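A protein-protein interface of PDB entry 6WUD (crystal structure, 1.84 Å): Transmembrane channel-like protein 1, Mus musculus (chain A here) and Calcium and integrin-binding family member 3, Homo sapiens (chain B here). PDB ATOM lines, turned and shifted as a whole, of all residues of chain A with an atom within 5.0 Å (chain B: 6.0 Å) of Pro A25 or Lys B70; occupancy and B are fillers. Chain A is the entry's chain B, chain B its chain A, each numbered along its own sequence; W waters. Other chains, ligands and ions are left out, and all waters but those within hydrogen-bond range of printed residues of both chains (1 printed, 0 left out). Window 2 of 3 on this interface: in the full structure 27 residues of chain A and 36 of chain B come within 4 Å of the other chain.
NZ of Lys B70 sits at hydrogen-bond distance from O of Gly A23 (3.2 Å).
The side-chain carboxylate of Asp B71 lies within hydrogen-bond range of the backbone NH of Asn A24.
The side-chain carboxylate (OD2) of Asp B71 sits close to the backbone carbonyl oxygen (O) of Gly A23 (3.2 Å).
NZ of Lys B70 is in salt-bridge range of OD2 of Asp B71.
The side-chain amide oxygen of Asn A24 is in hydrogen-bond range of the backbone NH of Glu A26 (2.7 Å).
N of Thr A27 lies within hydrogen-bond range of OD1 of Asn A24 (3.0 Å).
Among the printed residues, pairs that only touch across the chains: Gly A23 with Pro B67 (3.8 Å), Pro A25 with Lys B70 (3.7 Å), Pro A25 with Asp B71 (3.4 Å) and Ala A28 with Asp B71 (3.97 Å).
Printed residues of chain B within 4 Å of Gly A23: Pro B67, Lys B70 and Asp B71.
Of the printed residues of chain B, Asn A24 touches Asp B71 (3.2 Å).
Of chain B, only Lys B70 and Asp B71 come within 4 Å of Pro A25.
Printed residues of chain B within 4 Å of Ala A28: Asp B71.
Met B66 touches none of the printed residues of chain A.
Of the printed residues of chain A, Pro B67 touches Gly A23.
Leu B69 touches none of the printed residues of chain A.
Lys B70 touches just these residues of chain A: Gly A23 (3.2 Å) and Pro A25 (3.7 Å).
Printed residues of chain A within 4 Å of Asp B71: Gly A23, Asn A24, Pro A25 and Ala A28.
The nearest printed residue of chain B that does not touch Pro A25 is Pro B67 (8.1 Å).
The nearest residue of chain A that does not touch Lys B70 is Asn A24 (4.3 Å).
The nearest printed residue of chain B that does not touch Gly A23 is Glu B68 (5.7 Å).
Of the 7 printed residues of chain A, 4 touch a printed residue of chain B.
Hydrophobic or aromatic side chains of chain A within 4 Å of the printed part of chain B: Pro A25 and Ala A28.
Among the printed residues, 7 pairs touch across the chains.
Among the printed residues, no Asp or Glu carboxylate lies within 4 Å of a Lys or Arg side-chain nitrogen of the other chain.
Water W1 bridges the side-chain amino group (NZ) of Lys B70 and the backbone carbonyl oxygen (O) of Gly A23.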
ATOM      1  N   GLY A  23     -31.314  -9.500 -23.594  1.00  0.00           N
ATOM      2  CA  GLY A  23     -31.844  -9.843 -22.271  1.00  0.00           C
ATOM      3  C   GLY A  23     -31.853 -11.337 -21.986  1.00  0.00           C
ATOM      4  O   GLY A  23     -32.606 -11.810 -21.125  1.00  0.00           O
ATOM      5  N   ASN A  24     -31.003 -12.101 -22.687  1.00  0.00           N
ATOM      6  CA  ASN A  24     -30.842 -13.530 -22.474  1.00  0.00           C
ATOM      7  C   ASN A  24     -29.357 -13.814 -22.311  1.00  0.00           C
ATOM      8  O   ASN A  24     -28.536 -13.226 -23.044  1.00  0.00           O
ATOM      9  CB  ASN A  24     -31.391 -14.324 -23.673  1.00  0.00           C
ATOM     10  CG  ASN A  24     -31.093 -15.781 -23.581  1.00  0.00           C
ATOM     11  OD1 ASN A  24     -29.981 -16.228 -23.835  1.00  0.00           O
ATOM     12  ND2 ASN A  24     -32.107 -16.557 -23.185  1.00  0.00           N
ATOM     13  N   PRO A  25     -28.957 -14.670 -21.355  1.00  0.00           N
ATOM     14  CA  PRO A  25     -27.500 -14.846 -21.139  1.00  0.00           C
ATOM     15  C   PRO A  25     -26.786 -15.605 -22.263  1.00  0.00           C
ATOM     16  O   PRO A  25     -25.566 -15.401 -22.449  1.00  0.00           O
ATOM     17  CB  PRO A  25     -27.407 -15.609 -19.802  1.00  0.00           C
ATOM     18  CG  PRO A  25     -28.787 -16.299 -19.641  1.00  0.00           C
ATOM     19  CD  PRO A  25     -29.763 -15.304 -20.271  1.00  0.00           C
ATOM     20  N   GLU A  26     -27.476 -16.501 -22.963  1.00  0.00           N
ATOM     21  CA  GLU A  26     -26.838 -17.183 -24.092  1.00  0.00           C
ATOM     22  C   GLU A  26     -26.607 -16.204 -25.234  1.00  0.00           C
ATOM     23  O   GLU A  26     -25.519 -16.154 -25.839  1.00  0.00           O
ATOM     24  CB  GLU A  26     -27.669 -18.354 -24.598  1.00  0.00           C
ATOM     25  CG  GLU A  26     -27.791 -19.505 -23.648  1.00  0.00           C
ATOM     26  CD  GLU A  26     -28.750 -20.559 -24.183  1.00  0.00           C
ATOM     27  OE1 GLU A  26     -28.310 -21.402 -24.989  1.00  0.00           O
ATOM     28  OE2 GLU A  26     -29.948 -20.523 -23.823  1.00  0.00           O
ATOM     29  N   THR A  27     -27.636 -15.422 -25.555  1.00  0.00           N
ATOM     30  CA  THR A  27     -27.471 -14.386 -26.559  1.00  0.00           C
ATOM     31  C   THR A  27     -26.333 -13.460 -26.165  1.00  0.00           C
ATOM     32  O   THR A  27     -25.518 -13.072 -27.013  1.00  0.00           O
ATOM     33  CB  THR A  27     -28.790 -13.627 -26.735  1.00  0.00           C
ATOM     34  OG1 THR A  27     -29.810 -14.562 -27.085  1.00  0.00           O
ATOM     35  CG2 THR A  27     -28.658 -12.587 -27.821  1.00  0.00           C
ATOM     36  N   ALA A  28     -26.274 -13.076 -24.884  1.00  0.00           N
ATOM     37  CA  ALA A  28     -25.201 -12.199 -24.413  1.00  0.00           C
ATOM     38  C   ALA A  28     -23.828 -12.854 -24.574  1.00  0.00           C
ATOM     39  O   ALA A  28     -22.882 -12.218 -25.042  1.00  0.00           O
ATOM     40  CB  ALA A  28     -25.425 -11.807 -22.954  1.00  0.00           C
ATOM     41  N   ASP A  29     -23.700 -14.119 -24.167  1.00  0.00           N
ATOM     42  CA  ASP A  29     -22.447 -14.851 -24.341  1.00  0.00           C
ATOM     43  C   ASP A  29     -21.987 -14.821 -25.799  1.00  0.00           C
ATOM     44  O   ASP A  29     -20.819 -14.559 -26.085  1.00  0.00           O
ATOM     45  CB  ASP A  29     -22.613 -16.305 -23.888  1.00  0.00           C
ATOM     46  CG  ASP A  29     -21.279 -17.055 -23.781  1.00  0.00           C
ATOM     47  OD1 ASP A  29     -20.297 -16.557 -23.203  1.00  0.00           O
ATOM     48  OD2 ASP A  29     -21.224 -18.189 -24.252  1.00  0.00           O
ATOM     49  N   ILE B  63     -32.539  -3.268  -9.519  1.00  0.00           N
ATOM     50  CA  ILE B  63     -32.574  -2.601 -10.809  1.00  0.00           C
ATOM     51  C   ILE B  63     -31.677  -3.336 -11.804  1.00  0.00           C
ATOM     52  O   ILE B  63     -32.088  -3.656 -12.928  1.00  0.00           O
ATOM     53  CB  ILE B  63     -32.142  -1.123 -10.687  1.00  0.00           C
ATOM     54  CG1 ILE B  63     -33.003  -0.350  -9.717  1.00  0.00           C
ATOM     55  CG2 ILE B  63     -32.067  -0.534 -12.116  1.00  0.00           C
ATOM     56  CD1 ILE B  63     -34.315  -0.009 -10.209  1.00  0.00           C
ATOM     57  N   GLY B  64     -30.435  -3.607 -11.405  1.00  0.00           N
ATOM     58  CA  GLY B  64     -29.480  -4.250 -12.295  1.00  0.00           C
ATOM     59  C   GLY B  64     -29.825  -5.683 -12.649  1.00  0.00           C
ATOM     60  O   GLY B  64     -29.298  -6.214 -13.628  1.00  0.00           O
ATOM     61  N   SER B  65     -30.696  -6.323 -11.876  1.00  0.00           N
ATOM     62  CA  SER B  65     -31.094  -7.683 -12.161  1.00  0.00           C
ATOM     63  C   SER B  65     -32.410  -7.755 -12.931  1.00  0.00           C
ATOM     64  O   SER B  65     -32.816  -8.870 -13.288  1.00  0.00           O
ATOM     65  CB  SER B  65     -31.117  -8.509 -10.850  1.00  0.00           C
ATOM     66  OG  SER B  65     -31.933  -7.918  -9.902  1.00  0.00           O
ATOM     67  N   MET B  66     -33.006  -6.610 -13.297  1.00  0.00           N
ATOM     68  CA  MET B  66     -34.162  -6.584 -14.180  1.00  0.00           C
ATOM     69  C   MET B  66     -33.883  -7.241 -15.530  1.00  0.00           C
ATOM     70  O   MET B  66     -32.800  -7.076 -16.090  1.00  0.00           O
ATOM     71  CB  MET B  66     -34.570  -5.149 -14.514  1.00  0.00           C
ATOM     72  CG  MET B  66     -35.137  -4.271 -13.461  1.00  0.00           C
ATOM     73  SD  MET B  66     -35.361  -2.687 -14.387  1.00  0.00           S
ATOM     74  CE  MET B  66     -36.989  -3.037 -15.111  1.00  0.00           C
ATOM     75  N   PRO B  67     -34.883  -7.870 -16.152  1.00  0.00           N
ATOM     76  CA  PRO B  67     -34.622  -8.507 -17.454  1.00  0.00           C
ATOM     77  C   PRO B  67     -33.993  -7.553 -18.464  1.00  0.00           C
ATOM     78  O   PRO B  67     -33.118  -7.961 -19.253  1.00  0.00           O
ATOM     79  CB  PRO B  67     -36.006  -9.014 -17.895  1.00  0.00           C
ATOM     80  CG  PRO B  67     -36.832  -9.059 -16.615  1.00  0.00           C
ATOM     81  CD  PRO B  67     -36.272  -8.063 -15.674  1.00  0.00           C
ATOM     82  N   GLU B  68     -34.405  -6.290 -18.461  1.00  0.00           N
ATOM     83  CA  GLU B  68     -33.945  -5.361 -19.486  1.00  0.00           C
ATOM     84  C   GLU B  68     -32.512  -4.891 -19.291  1.00  0.00           C
ATOM     85  O   GLU B  68     -31.975  -4.243 -20.182  1.00  0.00           O
ATOM     86  CB  GLU B  68     -34.896  -4.152 -19.543  1.00  0.00           C
ATOM     87  CG  GLU B  68     -36.265  -4.510 -20.122  1.00  0.00           C
ATOM     88  CD  GLU B  68     -37.238  -5.157 -19.132  1.00  0.00           C
ATOM     89  OE1 GLU B  68     -36.882  -5.305 -17.929  1.00  0.00           O
ATOM     90  OE2 GLU B  68     -38.377  -5.505 -19.562  1.00  0.00           O
ATOM     91  N   LEU B  69     -31.907  -5.157 -18.131  1.00  0.00           N
ATOM     92  CA  LEU B  69     -30.562  -4.702 -17.828  1.00  0.00           C
ATOM     93  C   LEU B  69     -29.618  -5.817 -17.448  1.00  0.00           C
ATOM     94  O   LEU B  69     -28.397  -5.600 -17.493  1.00  0.00           O
ATOM     95  CB  LEU B  69     -30.555  -3.704 -16.661  1.00  0.00           C
ATOM     96  CG  LEU B  69     -31.049  -2.292 -17.006  1.00  0.00           C
ATOM     97  CD1 LEU B  69     -31.411  -1.597 -15.673  1.00  0.00           C
ATOM     98  CD2 LEU B  69     -30.061  -1.487 -17.857  1.00  0.00           C
ATOM     99  N   LYS B  70     -30.137  -6.962 -17.012  1.00  0.00           N
ATOM    100  CA  LYS B  70     -29.316  -7.947 -16.309  1.00  0.00           C
ATOM    101  C   LYS B  70     -28.130  -8.445 -17.141  1.00  0.00           C
ATOM    102  O   LYS B  70     -27.106  -8.843 -16.574  1.00  0.00           O
ATOM    103  CB  LYS B  70     -30.178  -9.138 -15.878  1.00  0.00           C
ATOM    104  CG  LYS B  70     -30.659 -10.052 -17.035  1.00  0.00           C
ATOM    105  CD  LYS B  70     -31.716 -10.986 -16.519  1.00  0.00           C
ATOM    106  CE  LYS B  70     -32.397 -11.789 -17.619  1.00  0.00           C
ATOM    107  NZ  LYS B  70     -31.628 -12.812 -18.289  1.00  0.00           N
ATOM    108  N   ASP B  71     -28.254  -8.494 -18.468  1.00  0.00           N
ATOM    109  CA  ASP B  71     -27.195  -9.000 -19.329  1.00  0.00           C
ATOM    110  C   ASP B  71     -26.334  -7.898 -19.938  1.00  0.00           C
ATOM    111  O   ASP B  71     -25.414  -8.193 -20.713  1.00  0.00           O
ATOM    112  CB  ASP B  71     -27.804  -9.904 -20.407  1.00  0.00           C
ATOM    113  CG  ASP B  71     -28.438 -11.139 -19.810  1.00  0.00           C
ATOM    114  OD1 ASP B  71     -27.738 -12.003 -19.218  1.00  0.00           O
ATOM    115  OD2 ASP B  71     -29.662 -11.230 -19.922  1.00  0.00           O
ATOM    116  N   ASN B  72     -26.562  -6.661 -19.559  1.00  0.00           N
ATOM    117  CA  ASN B  72     -25.808  -5.529 -20.105  1.00  0.00           C
ATOM    118  C   ASN B  72     -24.523  -5.360 -19.305  1.00  0.00           C
ATOM    119  O   ASN B  72     -24.607  -5.146 -18.086  1.00  0.00           O
ATOM    120  CB  ASN B  72     -26.653  -4.271 -20.016  1.00  0.00           C
ATOM    121  CG  ASN B  72     -26.096  -3.115 -20.809  1.00  0.00           C
ATOM    122  OD1 ASN B  72     -24.883  -2.873 -20.812  1.00  0.00           O
ATOM    123  ND2 ASN B  72     -26.966  -2.415 -21.516  1.00  0.00           N
ATOM    124  N   ARG B  75     -24.627  -2.207 -17.089  1.00  0.00           N
ATOM    125  CA  ARG B  75     -25.836  -2.017 -16.292  1.00  0.00           C
ATOM    126  C   ARG B  75     -25.581  -1.186 -15.034  1.00  0.00           C
ATOM    127  O   ARG B  75     -26.430  -0.364 -14.648  1.00  0.00           O
ATOM    128  CB  ARG B  75     -26.448  -3.388 -15.917  1.00  0.00           C
ATOM    129  CG  ARG B  75     -25.581  -4.330 -15.071  1.00  0.00           C
ATOM    130  CD  ARG B  75     -26.159  -5.779 -15.142  1.00  0.00           C
ATOM    131  NE  ARG B  75     -25.327  -6.659 -14.342  1.00  0.00           N
ATOM    132  CZ  ARG B  75     -24.142  -7.099 -14.703  1.00  0.00           C
ATOM    133  NH1 ARG B  75     -23.683  -6.811 -15.919  1.00  0.00           N
ATOM    134  NH2 ARG B  75     -23.446  -7.864 -13.866  1.00  0.00           N
HETATM  135  O   HOH W   1     -33.180 -14.684 -19.463  1.00  0.00           O
